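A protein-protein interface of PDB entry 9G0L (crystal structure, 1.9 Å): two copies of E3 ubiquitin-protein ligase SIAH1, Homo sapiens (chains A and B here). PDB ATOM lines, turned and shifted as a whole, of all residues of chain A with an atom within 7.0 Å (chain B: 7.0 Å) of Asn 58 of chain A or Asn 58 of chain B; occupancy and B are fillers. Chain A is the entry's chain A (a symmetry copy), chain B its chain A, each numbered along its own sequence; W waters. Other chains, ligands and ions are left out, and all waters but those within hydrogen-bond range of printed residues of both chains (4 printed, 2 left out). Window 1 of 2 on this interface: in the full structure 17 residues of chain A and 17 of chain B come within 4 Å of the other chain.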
ATOM      1  N   PRO A  25      19.640 -14.865  20.410  1.00  0.00           N
ATOM      2  CA  PRO A  25      18.855 -16.073  20.676  1.00  0.00           C
ATOM      3  C   PRO A  25      17.352 -15.798  20.769  1.00  0.00           C
ATOM      4  O   PRO A  25      16.931 -14.848  21.424  1.00  0.00           O
ATOM      5  CB  PRO A  25      19.391 -16.550  22.019  1.00  0.00           C
ATOM      6  CG  PRO A  25      19.921 -15.332  22.680  1.00  0.00           C
ATOM      7  CD  PRO A  25      20.287 -14.336  21.623  1.00  0.00           C
ATOM      8  N   ILE A  26      16.554 -16.643  20.130  1.00  0.00           N
ATOM      9  CA  ILE A  26      15.123 -16.416  20.014  1.00  0.00           C
ATOM     10  C   ILE A  26      14.416 -17.254  21.081  1.00  0.00           C
ATOM     11  O   ILE A  26      14.484 -18.489  21.052  1.00  0.00           O
ATOM     12  CB  ILE A  26      14.618 -16.777  18.608  1.00  0.00           C
ATOM     13  CG1 ILE A  26      15.126 -15.796  17.559  1.00  0.00           C
ATOM     14  CG2 ILE A  26      13.090 -16.762  18.579  1.00  0.00           C
ATOM     15  CD1 ILE A  26      14.760 -16.228  16.168  1.00  0.00           C
ATOM     16  N   LEU A  27      13.704 -16.592  21.996  1.00  0.00           N
ATOM     17  CA  LEU A  27      12.914 -17.222  23.057  1.00  0.00           C
ATOM     18  C   LEU A  27      11.424 -17.111  22.728  1.00  0.00           C
ATOM     19  O   LEU A  27      11.017 -16.264  21.933  1.00  0.00           O
ATOM     20  CB  LEU A  27      13.193 -16.543  24.403  1.00  0.00           C
ATOM     21  CG  LEU A  27      14.640 -16.527  24.889  1.00  0.00           C
ATOM     22  CD1 LEU A  27      14.729 -15.991  26.291  1.00  0.00           C
ATOM     23  CD2 LEU A  27      15.217 -17.942  24.806  1.00  0.00           C
ATOM     24  N   GLN A  28      10.602 -17.962  23.350  1.00  0.00           N
ATOM     25  CA  GLN A  28       9.159 -17.874  23.138  1.00  0.00           C
ATOM     26  C   GLN A  28       8.386 -18.407  24.336  1.00  0.00           C
ATOM     27  O   GLN A  28       8.908 -19.164  25.151  1.00  0.00           O
ATOM     28  CB  GLN A  28       8.727 -18.660  21.903  1.00  0.00           C
ATOM     29  CG  GLN A  28       8.892 -20.155  22.096  1.00  0.00           C
ATOM     30  CD  GLN A  28       8.209 -20.968  21.007  1.00  0.00           C
ATOM     31  OE1 GLN A  28       8.516 -20.842  19.811  1.00  0.00           O
ATOM     32  NE2 GLN A  28       7.267 -21.796  21.414  1.00  0.00           N
ATOM     33  N   GLN A  30       5.023 -20.592  25.972  1.00  0.00           N
ATOM     34  CA  GLN A  30       4.471 -21.929  25.755  1.00  0.00           C
ATOM     35  C   GLN A  30       3.676 -22.044  24.453  1.00  0.00           C
ATOM     36  O   GLN A  30       3.669 -23.105  23.828  1.00  0.00           O
ATOM     37  CB  GLN A  30       3.574 -22.306  26.939  1.00  0.00           C
ATOM     38  CG  GLN A  30       2.787 -23.610  26.762  1.00  0.00           C
ATOM     39  CD  GLN A  30       3.626 -24.816  27.110  1.00  0.00           C
ATOM     40  OE1 GLN A  30       4.589 -24.715  27.877  1.00  0.00           O
ATOM     41  NE2 GLN A  30       3.277 -25.967  26.541  1.00  0.00           N
ATOM     42  N   SER A  31       2.964 -20.988  24.055  1.00  0.00           N
ATOM     43  CA  SER A  31       2.077 -21.031  22.891  1.00  0.00           C
ATOM     44  C   SER A  31       2.710 -20.463  21.608  1.00  0.00           C
ATOM     45  O   SER A  31       2.013 -20.337  20.584  1.00  0.00           O
ATOM     46  CB  SER A  31       0.766 -20.313  23.223  1.00  0.00           C
ATOM     47  OG  SER A  31       0.183 -20.856  24.411  1.00  0.00           O
ATOM     48  N   GLY A  32       4.001 -20.141  21.634  1.00  0.00           N
ATOM     49  CA  GLY A  32       4.749 -19.800  20.421  1.00  0.00           C
ATOM     50  C   GLY A  32       4.892 -18.326  20.056  1.00  0.00           C
ATOM     51  O   GLY A  32       5.243 -18.023  18.909  1.00  0.00           O
ATOM     52  N   LEU A  34       6.648 -14.544  20.251  1.00  0.00           N
ATOM     53  CA  LEU A  34       8.017 -14.044  20.317  1.00  0.00           C
ATOM     54  C   LEU A  34       8.021 -12.646  20.930  1.00  0.00           C
ATOM     55  O   LEU A  34       7.052 -11.899  20.792  1.00  0.00           O
ATOM     56  CB  LEU A  34       8.627 -13.994  18.913  1.00  0.00           C
ATOM     57  CG  LEU A  34       8.711 -15.233  18.006  1.00  0.00           C
ATOM     58  CD1 LEU A  34       9.713 -14.979  16.896  1.00  0.00           C
ATOM     59  CD2 LEU A  34       9.119 -16.479  18.737  1.00  0.00           C
ATOM     60  N   SER A  55      11.458 -19.013  28.867  1.00  0.00           N
ATOM     61  CA  SER A  55      12.727 -18.985  28.156  1.00  0.00           C
ATOM     62  C   SER A  55      12.861 -20.243  27.326  1.00  0.00           C
ATOM     63  O   SER A  55      13.960 -20.780  27.149  1.00  0.00           O
ATOM     64  CB  SER A  55      13.896 -18.854  29.128  1.00  0.00           C
ATOM     65  OG  SER A  55      13.870 -19.949  30.013  1.00  0.00           O
ATOM     66  N   ILE A  56      11.735 -20.725  26.805  1.00  0.00           N
ATOM     67  CA  ILE A  56      11.761 -21.792  25.825  1.00  0.00           C
ATOM     68  C   ILE A  56      12.552 -21.305  24.621  1.00  0.00           C
ATOM     69  O   ILE A  56      12.405 -20.162  24.191  1.00  0.00           O
ATOM     70  CB  ILE A  56      10.326 -22.156  25.418  1.00  0.00           C
ATOM     71  CG1 ILE A  56       9.548 -22.721  26.616  1.00  0.00           C
ATOM     72  CG2 ILE A  56      10.349 -23.118  24.260  1.00  0.00           C
ATOM     73  CD1 ILE A  56       8.092 -22.729  26.373  1.00  0.00           C
ATOM     74  N   ARG A  57      13.401 -22.158  24.077  1.00  0.00           N
ATOM     75  CA  ARG A  57      14.323 -21.754  23.024  1.00  0.00           C
ATOM     76  C   ARG A  57      13.734 -22.151  21.671  1.00  0.00           C
ATOM     77  O   ARG A  57      13.400 -23.318  21.455  1.00  0.00           O
ATOM     78  CB  ARG A  57      15.692 -22.396  23.245  1.00  0.00           C
ATOM     79  CG  ARG A  57      16.717 -21.975  22.225  1.00  0.00           C
ATOM     80  CD  ARG A  57      17.546 -20.792  22.682  1.00  0.00           C
ATOM     81  NE  ARG A  57      18.656 -20.586  21.765  1.00  0.00           N
ATOM     82  CZ  ARG A  57      19.891 -21.051  21.906  1.00  0.00           C
ATOM     83  NH1 ARG A  57      20.309 -21.625  23.041  1.00  0.00           N
ATOM     84  NH2 ARG A  57      20.742 -20.913  20.896  1.00  0.00           N
ATOM     85  N   ASN A  58      13.604 -21.188  20.758  1.00  0.00           N
ATOM     86  CA  ASN A  58      13.168 -21.505  19.393  1.00  0.00           C
ATOM     87  C   ASN A  58      14.404 -21.646  18.503  1.00  0.00           C
ATOM     88  O   ASN A  58      14.791 -20.738  17.769  1.00  0.00           O
ATOM     89  CB  ASN A  58      12.159 -20.464  18.874  1.00  0.00           C
ATOM     90  CG  ASN A  58      11.399 -20.970  17.663  1.00  0.00           C
ATOM     91  OD1 ASN A  58      11.935 -21.765  16.899  1.00  0.00           O
ATOM     92  ND2 ASN A  58      10.132 -20.573  17.518  1.00  0.00           N
ATOM     93  N   LEU A  59      15.047 -22.819  18.591  1.00  0.00           N
ATOM     94  CA  LEU A  59      16.259 -23.063  17.813  1.00  0.00           C
ATOM     95  C   LEU A  59      15.963 -23.052  16.319  1.00  0.00           C
ATOM     96  O   LEU A  59      16.796 -22.607  15.527  1.00  0.00           O
ATOM     97  CB  LEU A  59      16.889 -24.402  18.180  1.00  0.00           C
ATOM     98  CG  LEU A  59      17.587 -24.600  19.519  1.00  0.00           C
ATOM     99  CD1 LEU A  59      17.950 -26.051  19.617  1.00  0.00           C
ATOM    100  CD2 LEU A  59      18.831 -23.713  19.639  1.00  0.00           C
ATOM    101  N   ALA A  60      14.809 -23.587  15.915  1.00  0.00           N
ATOM    102  CA  ALA A  60      14.494 -23.691  14.491  1.00  0.00           C
ATOM    103  C   ALA A  60      14.414 -22.315  13.831  1.00  0.00           C
ATOM    104  O   ALA A  60      14.957 -22.100  12.741  1.00  0.00           O
ATOM    105  CB  ALA A  60      13.185 -24.457  14.300  1.00  0.00           C
ATOM    106  N   MET A  61      13.717 -21.380  14.469  1.00  0.00           N
ATOM    107  CA  MET A  61      13.669 -19.996  13.999  1.00  0.00           C
ATOM    108  C   MET A  61      15.043 -19.356  13.932  1.00  0.00           C
ATOM    109  O   MET A  61      15.296 -18.540  13.034  1.00  0.00           O
ATOM    110  CB  MET A  61      12.759 -19.199  14.921  1.00  0.00           C
ATOM    111  CG  MET A  61      11.302 -19.126  14.506  1.00  0.00           C
ATOM    112  SD  MET A  61      10.889 -19.055  12.717  1.00  0.00           S
ATOM    113  CE  MET A  61      10.858 -17.309  12.494  1.00  0.00           C
ATOM    114  N   GLU A  62      15.920 -19.637  14.910  1.00  0.00           N
ATOM    115  CA  GLU A  62      17.291 -19.140  14.804  1.00  0.00           C
ATOM    116  C   GLU A  62      17.958 -19.664  13.552  1.00  0.00           C
ATOM    117  O   GLU A  62      18.753 -18.957  12.923  1.00  0.00           O
ATOM    118  CB  GLU A  62      18.118 -19.526  16.026  1.00  0.00           C
ATOM    119  CG  GLU A  62      17.623 -18.901  17.327  1.00  0.00           C
ATOM    120  CD  GLU A  62      18.370 -19.433  18.547  1.00  0.00           C
ATOM    121  OE1 GLU A  62      19.396 -20.131  18.395  1.00  0.00           O
ATOM    122  OE2 GLU A  62      17.926 -19.153  19.661  1.00  0.00           O
ATOM    123  N   LYS A  63      17.671 -20.909  13.176  1.00  0.00           N
ATOM    124  CA  LYS A  63      18.299 -21.432  11.966  1.00  0.00           C
ATOM    125  C   LYS A  63      17.713 -20.787  10.712  1.00  0.00           C
ATOM    126  O   LYS A  63      18.448 -20.492   9.760  1.00  0.00           O
ATOM    127  CB  LYS A  63      18.169 -22.950  11.902  1.00  0.00           C
ATOM    128  CG  LYS A  63      19.125 -23.644  12.895  1.00  0.00           C
ATOM    129  CD  LYS A  63      18.930 -25.136  12.972  1.00  0.00           C
ATOM    130  CE  LYS A  63      19.722 -25.712  14.160  1.00  0.00           C
ATOM    131  NZ  LYS A  63      20.024 -24.634  15.143  1.00  0.00           N
ATOM    132  N   PRO B  25       0.617 -29.260  12.662  1.00  0.00           N
ATOM    133  CA  PRO B  25       1.114 -28.391  13.731  1.00  0.00           C
ATOM    134  C   PRO B  25       2.482 -28.824  14.263  1.00  0.00           C
ATOM    135  O   PRO B  25       2.707 -30.005  14.518  1.00  0.00           O
ATOM    136  CB  PRO B  25       0.054 -28.528  14.815  1.00  0.00           C
ATOM    137  CG  PRO B  25      -0.568 -29.855  14.583  1.00  0.00           C
ATOM    138  CD  PRO B  25      -0.395 -30.217  13.140  1.00  0.00           C
ATOM    139  N   ILE B  26       3.378 -27.864  14.446  1.00  0.00           N
ATOM    140  CA  ILE B  26       4.757 -28.152  14.807  1.00  0.00           C
ATOM    141  C   ILE B  26       4.907 -27.967  16.317  1.00  0.00           C
ATOM    142  O   ILE B  26       4.735 -26.855  16.831  1.00  0.00           O
ATOM    143  CB  ILE B  26       5.730 -27.242  14.041  1.00  0.00           C
ATOM    144  CG1 ILE B  26       5.768 -27.581  12.557  1.00  0.00           C
ATOM    145  CG2 ILE B  26       7.143 -27.392  14.605  1.00  0.00           C
ATOM    146  CD1 ILE B  26       6.602 -26.600  11.782  1.00  0.00           C
ATOM    147  N   LEU B  27       5.269 -29.040  17.025  1.00  0.00           N
ATOM    148  CA  LEU B  27       5.519 -29.044  18.469  1.00  0.00           C
ATOM    149  C   LEU B  27       7.023 -29.138  18.734  1.00  0.00           C
ATOM    150  O   LEU B  27       7.788 -29.566  17.869  1.00  0.00           O
ATOM    151  CB  LEU B  27       4.807 -30.230  19.128  1.00  0.00           C
ATOM    152  CG  LEU B  27       3.294 -30.324  18.949  1.00  0.00           C
ATOM    153  CD1 LEU B  27       2.721 -31.428  19.792  1.00  0.00           C
ATOM    154  CD2 LEU B  27       2.659 -28.978  19.303  1.00  0.00           C
ATOM    155  N   GLN B  28       7.451 -28.751  19.939  1.00  0.00           N
ATOM    156  CA  GLN B  28       8.864 -28.873  20.290  1.00  0.00           C
ATOM    157  C   GLN B  28       9.055 -29.024  21.792  1.00  0.00           C
ATOM    158  O   GLN B  28       8.185 -28.675  22.587  1.00  0.00           O
ATOM    159  CB  GLN B  28       9.662 -27.657  19.827  1.00  0.00           C
ATOM    160  CG  GLN B  28       9.289 -26.407  20.599  1.00  0.00           C
ATOM    161  CD  GLN B  28      10.258 -25.258  20.362  1.00  0.00           C
ATOM    162  OE1 GLN B  28      10.453 -24.795  19.228  1.00  0.00           O
ATOM    163  NE2 GLN B  28      10.881 -24.804  21.432  1.00  0.00           N
ATOM    164  N   GLN B  30      11.285 -28.168  25.405  1.00  0.00           N
ATOM    165  CA  GLN B  30      11.743 -26.941  26.055  1.00  0.00           C
ATOM    166  C   GLN B  30      12.966 -26.323  25.373  1.00  0.00           C
ATOM    167  O   GLN B  30      13.111 -25.101  25.360  1.00  0.00           O
ATOM    168  CB  GLN B  30      12.068 -27.235  27.524  1.00  0.00           C
ATOM    169  CG  GLN B  30      12.730 -26.078  28.282  1.00  0.00           C
ATOM    170  CD  GLN B  30      11.707 -25.087  28.784  1.00  0.00           C
ATOM    171  OE1 GLN B  30      10.537 -25.432  28.979  1.00  0.00           O
ATOM    172  NE2 GLN B  30      12.135 -23.845  28.989  1.00  0.00           N
ATOM    173  N   SER B  31      13.877 -27.146  24.850  1.00  0.00           N
ATOM    174  CA  SER B  31      15.138 -26.665  24.282  1.00  0.00           C
ATOM    175  C   SER B  31      15.112 -26.520  22.751  1.00  0.00           C
ATOM    176  O   SER B  31      16.161 -26.233  22.143  1.00  0.00           O
ATOM    177  CB  SER B  31      16.281 -27.580  24.730  1.00  0.00           C
ATOM    178  OG  SER B  31      16.300 -27.699  26.156  1.00  0.00           O
ATOM    179  N   GLY B  32      13.951 -26.689  22.123  1.00  0.00           N
ATOM    180  CA  GLY B  32      13.771 -26.364  20.705  1.00  0.00           C
ATOM    181  C   GLY B  32      13.926 -27.488  19.685  1.00  0.00           C
ATOM    182  O   GLY B  32      14.080 -27.199  18.493  1.00  0.00           O
ATOM    183  N   LEU B  34      12.613 -30.750  17.435  1.00  0.00           N
ATOM    184  CA  LEU B  34      11.383 -31.088  16.728  1.00  0.00           C
ATOM    185  C   LEU B  34      11.279 -32.604  16.580  1.00  0.00           C
ATOM    186  O   LEU B  34      12.294 -33.297  16.506  1.00  0.00           O
ATOM    187  CB  LEU B  34      11.374 -30.432  15.345  1.00  0.00           C
ATOM    188  CG  LEU B  34      11.528 -28.914  15.150  1.00  0.00           C
ATOM    189  CD1 LEU B  34      11.066 -28.535  13.756  1.00  0.00           C
ATOM    190  CD2 LEU B  34      10.747 -28.105  16.145  1.00  0.00           C
ATOM    191  N   SER B  55       4.420 -30.252  24.503  1.00  0.00           N
ATOM    192  CA  SER B  55       3.536 -29.827  23.428  1.00  0.00           C
ATOM    193  C   SER B  55       3.613 -28.323  23.285  1.00  0.00           C
ATOM    194  O   SER B  55       2.621 -27.659  22.961  1.00  0.00           O
ATOM    195  CB  SER B  55       2.100 -30.272  23.693  1.00  0.00           C
ATOM    196  OG  SER B  55       1.672 -29.709  24.911  1.00  0.00           O
ATOM    197  N   ILE B  56       4.799 -27.770  23.525  1.00  0.00           N
ATOM    198  CA  ILE B  56       5.051 -26.377  23.216  1.00  0.00           C
ATOM    199  C   ILE B  56       4.842 -26.181  21.723  1.00  0.00           C
ATOM    200  O   ILE B  56       5.256 -27.010  20.915  1.00  0.00           O
ATOM    201  CB  ILE B  56       6.488 -26.010  23.614  1.00  0.00           C
ATOM    202  CG1 ILE B  56       6.679 -26.133  25.133  1.00  0.00           C
ATOM    203  CG2 ILE B  56       6.822 -24.629  23.117  1.00  0.00           C
ATOM    204  CD1 ILE B  56       8.107 -26.159  25.508  1.00  0.00           C
ATOM    205  N   ARG B  57       4.191 -25.095  21.347  1.00  0.00           N
ATOM    206  CA  ARG B  57       3.795 -24.881  19.961  1.00  0.00           C
ATOM    207  C   ARG B  57       4.821 -23.971  19.287  1.00  0.00           C
ATOM    208  O   ARG B  57       5.096 -22.873  19.776  1.00  0.00           O
ATOM    209  CB  ARG B  57       2.392 -24.280  19.899  1.00  0.00           C
ATOM    210  CG  ARG B  57       1.891 -24.087  18.492  1.00  0.00           C
ATOM    211  CD  ARG B  57       1.070 -25.259  17.997  1.00  0.00           C
ATOM    212  NE  ARG B  57       0.429 -24.914  16.737  1.00  0.00           N
ATOM    213  CZ  ARG B  57      -0.803 -24.446  16.582  1.00  0.00           C
ATOM    214  NH1 ARG B  57      -1.682 -24.414  17.590  1.00  0.00           N
ATOM    215  NH2 ARG B  57      -1.176 -24.024  15.380  1.00  0.00           N
ATOM    216  N   ASN B  58       5.390 -24.420  18.168  1.00  0.00           N
ATOM    217  CA  ASN B  58       6.289 -23.559  17.388  1.00  0.00           C
ATOM    218  C   ASN B  58       5.488 -22.908  16.260  1.00  0.00           C
ATOM    219  O   ASN B  58       5.508 -23.339  15.108  1.00  0.00           O
ATOM    220  CB  ASN B  58       7.517 -24.343  16.890  1.00  0.00           C
ATOM    221  CG  ASN B  58       8.635 -23.419  16.446  1.00  0.00           C
ATOM    222  OD1 ASN B  58       8.361 -22.314  15.989  1.00  0.00           O
ATOM    223  ND2 ASN B  58       9.890 -23.828  16.642  1.00  0.00           N
ATOM    224  N   LEU B  59       4.750 -21.847  16.616  1.00  0.00           N
ATOM    225  CA  LEU B  59       3.917 -21.157  15.633  1.00  0.00           C
ATOM    226  C   LEU B  59       4.769 -20.515  14.546  1.00  0.00           C
ATOM    227  O   LEU B  59       4.358 -20.466  13.386  1.00  0.00           O
ATOM    228  CB  LEU B  59       3.066 -20.079  16.293  1.00  0.00           C
ATOM    229  CG  LEU B  59       1.887 -20.445  17.184  1.00  0.00           C
ATOM    230  CD1 LEU B  59       1.373 -19.170  17.783  1.00  0.00           C
ATOM    231  CD2 LEU B  59       0.787 -21.162  16.393  1.00  0.00           C
ATOM    232  N   ALA B  60       5.932 -19.971  14.916  1.00  0.00           N
ATOM    233  CA  ALA B  60       6.764 -19.260  13.945  1.00  0.00           C
ATOM    234  C   ALA B  60       7.228 -20.185  12.820  1.00  0.00           C
ATOM    235  O   ALA B  60       7.175 -19.825  11.638  1.00  0.00           O
ATOM    236  CB  ALA B  60       7.962 -18.625  14.650  1.00  0.00           C
ATOM    237  N   MET B  61       7.711 -21.371  13.175  1.00  0.00           N
ATOM    238  CA  MET B  61       8.074 -22.387  12.187  1.00  0.00           C
ATOM    239  C   MET B  61       6.903 -22.787  11.307  1.00  0.00           C
ATOM    240  O   MET B  61       7.100 -23.074  10.118  1.00  0.00           O
ATOM    241  CB  MET B  61       8.627 -23.601  12.916  1.00  0.00           C
ATOM    242  CG  MET B  61      10.131 -23.620  13.115  1.00  0.00           C
ATOM    243  SD  MET B  61      11.211 -22.908  11.811  1.00  0.00           S
ATOM    244  CE  MET B  61      11.498 -24.353  10.849  1.00  0.00           C
ATOM    245  N   GLU B  62       5.693 -22.898  11.879  1.00  0.00           N
ATOM    246  CA  GLU B  62       4.527 -23.154  11.034  1.00  0.00           C
ATOM    247  C   GLU B  62       4.350 -22.055  10.011  1.00  0.00           C
ATOM    248  O   GLU B  62       3.936 -22.315   8.877  1.00  0.00           O
ATOM    249  CB  GLU B  62       3.256 -23.288  11.867  1.00  0.00           C
ATOM    250  CG  GLU B  62       3.265 -24.483  12.817  1.00  0.00           C
ATOM    251  CD  GLU B  62       2.055 -24.495  13.745  1.00  0.00           C
ATOM    252  OE1 GLU B  62       1.105 -23.708  13.544  1.00  0.00           O
ATOM    253  OE2 GLU B  62       2.057 -25.294  14.683  1.00  0.00           O
ATOM    254  N   LYS B  63       4.636 -20.810  10.389  1.00  0.00           N
ATOM    255  CA  LYS B  63       4.480 -19.734   9.415  1.00  0.00           C
ATOM    256  C   LYS B  63       5.568 -19.790   8.344  1.00  0.00           C
ATOM    257  O   LYS B  63       5.293 -19.545   7.162  1.00  0.00           O
ATOM    258  CB  LYS B  63       4.475 -18.375  10.106  1.00  0.00           C
ATOM    259  CG  LYS B  63       3.145 -18.120  10.846  1.00  0.00           C
ATOM    260  CD  LYS B  63       3.147 -16.854  11.663  1.00  0.00           C
ATOM    261  CE  LYS B  63       1.903 -16.808  12.570  1.00  0.00           C
ATOM    262  NZ  LYS B  63       1.351 -18.180  12.748  1.00  0.00           N
HETATM  263  O   HOH W   1      10.616 -21.517  30.157  1.00  0.00           O
HETATM  264  O   HOH W   2       1.118 -25.986  24.505  1.00  0.00           O
HETATM  265  O   HOH W   3       4.444 -28.708  27.005  1.00  0.00           O
HETATM  266  O   HOH W   4      14.902 -23.112  28.206  1.00  0.00           O
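Ser 31 of chain A touches Arg 57 of chain B, and with the chains exchanged Arg 57 of chain A touches Ser 31 of chain B.
Gly 32 of chain A touches Arg 57 of chain B, and with the chains exchanged Arg 57 of chain A touches Gly 32 of chain B.
Gly 32 of chain A touches Leu 59 of chain B, and with the chains exchanged Leu 59 of chain A touches Gly 32 of chain B.
Asn 58 of chain B touches its own counterpart, Asn 58 of chain A.
17 positions are printed for both chains.
Of the 21 pairs that touch across the chains among the printed residues, 21 have their exchanged pair printed and touching as well.
Among the printed residues, merely in contact across the chains: Leu 59 of chain A with Ser 31 of chain B, Ser 31 of chain A with Leu 59 of chain B, Ile 56 of chain A with Gln 28 of chain B, Gln 28 of chain A with Ile 56 of chain B, Met 61 of chain A with Ala 60 of chain B, Ala 60 of chain A with Met 61 of chain B, Ile 56 of chain A with Ile 56 of chain B, Gln 30 of chain A with Ile 56 of chain B, Ile 56 of chain A with Gln 30 of chain B, Ser 31 of chain A with Arg 57 of chain B, Arg 57 of chain A with Ser 31 of chain B, Met 61 of chain A with Met 61 of chain B, Gly 32 of chain A with Leu 59 of chain B and Leu 59 of chain A with Gly 32 of chain B.
The side-chain amide nitrogen (NE2) of Gln 28 of chain B sits at hydrogen-bond distance from the backbone carbonyl oxygen (O) of Arg 57 of chain A, 2.9 Å away.
The backbone carbonyl oxygen (O) of Gln 30 of chain B lies within hydrogen-bond range of the backbone NH (N) of Arg 57 of chain A, 3.2 Å away.
O of Arg 57 of chain A lies close to N of Gly 32 of chain B, at 3.5 Å.
The backbone carbonyl oxygen (O) of Arg 57 of chain B is in hydrogen-bond range of the side-chain amide nitrogen (NE2) of Gln 28 of chain A (2.9 Å).
N of Arg 57 of chain B is in hydrogen-bond range of O of Gln 30 of chain A, at 3.2 Å.
The backbone carbonyl oxygen (O) of Arg 57 of chain B sits close to the backbone NH (N) of Gly 32 of chain A, 3.5 Å away.
OD1 of Asn 58 of chain B lies within hydrogen-bond range of ND2 of Asn 58 of chain A.
Of the 17 printed residues of chain A, 10 touch a printed residue of chain B.
Hydrophobic or aromatic side chains of chain A that line the printed part of chain B: Ile 56, Leu 59, Ala 60 and Met 61.
Among the printed residues, 21 pairs touch across the chains.
N of Asn 58 of chain B sits at hydrogen-bond distance from O of Ile 26 of chain B (2.9 Å).
The side-chain carboxylate (OE2) of Glu 62 of chain B lies within salt-bridge range of the guanidinium group (NE) of Arg 57 of chain B (2.6 Å).
OD1 of Asn 58 of chain B sits at hydrogen-bond distance from N of Met 61 of chain B.
The backbone NH (N) of Gln 28 of chain A lies within hydrogen-bond range of the backbone carbonyl oxygen (O) of Ile 56 of chain A (3.0 Å).
OE2 of Glu 62 of chain A lies within salt-bridge range of NE of Arg 57 of chain A (2.6 Å).
The backbone NH (N) of Met 61 of chain A sits at hydrogen-bond distance from the side-chain amide oxygen (OD1) of Asn 58 of chain A.
Of the printed residues of chain B, Asn 58 of chain A touches Asn 58 (2.9 Å).
Of chain A, only Asn 58 comes within 4 Å of Asn 58 of chain B.
Printed residues of chain A within 4 Å of Ala 60 of chain B: Met 61.
Of the printed residues of chain A, Gln 28 of chain B touches Ile 56 (3.3 Å) and Arg 57 (2.9 Å).
Of the printed residues of chain A, Ser 31 of chain B touches Arg 57 and Leu 59.
Of the printed residues of chain A, Met 61 of chain B touches Ala 60 and Met 61.
Of the printed residues of chain B, Ala 60 of chain A touches Met 61.
The nearest printed residue of chain B that does not touch Asn 58 of chain A is Ala 60 of chain B (4.1 Å).
The nearest printed residue of chain A that does not touch Asn 58 of chain B is Ala 60 of chain A (4.1 Å).
The nearest printed residue of chain B that does not touch Ser 31 of chain A is Ile 56 of chain B (5.4 Å).
Water W2 bridges O of Ser 55 of chain B and NE2 of Gln 30 of chain A.
Water W4 lies within hydrogen-bond range of O of Ser 55 of chain A (2.7 Å) and NE2 of Gln 30 of chain B (3.0 Å).
Water W3 bridges the backbone NH (N) of Ser 55 of chain B and the side-chain amide nitrogen (NE2) of Gln 30 of chain A.
Water W1 bridges N of Ser 55 of chain A (2.9 Å) and NE2 of Gln 30 of chain B (3.0 Å).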
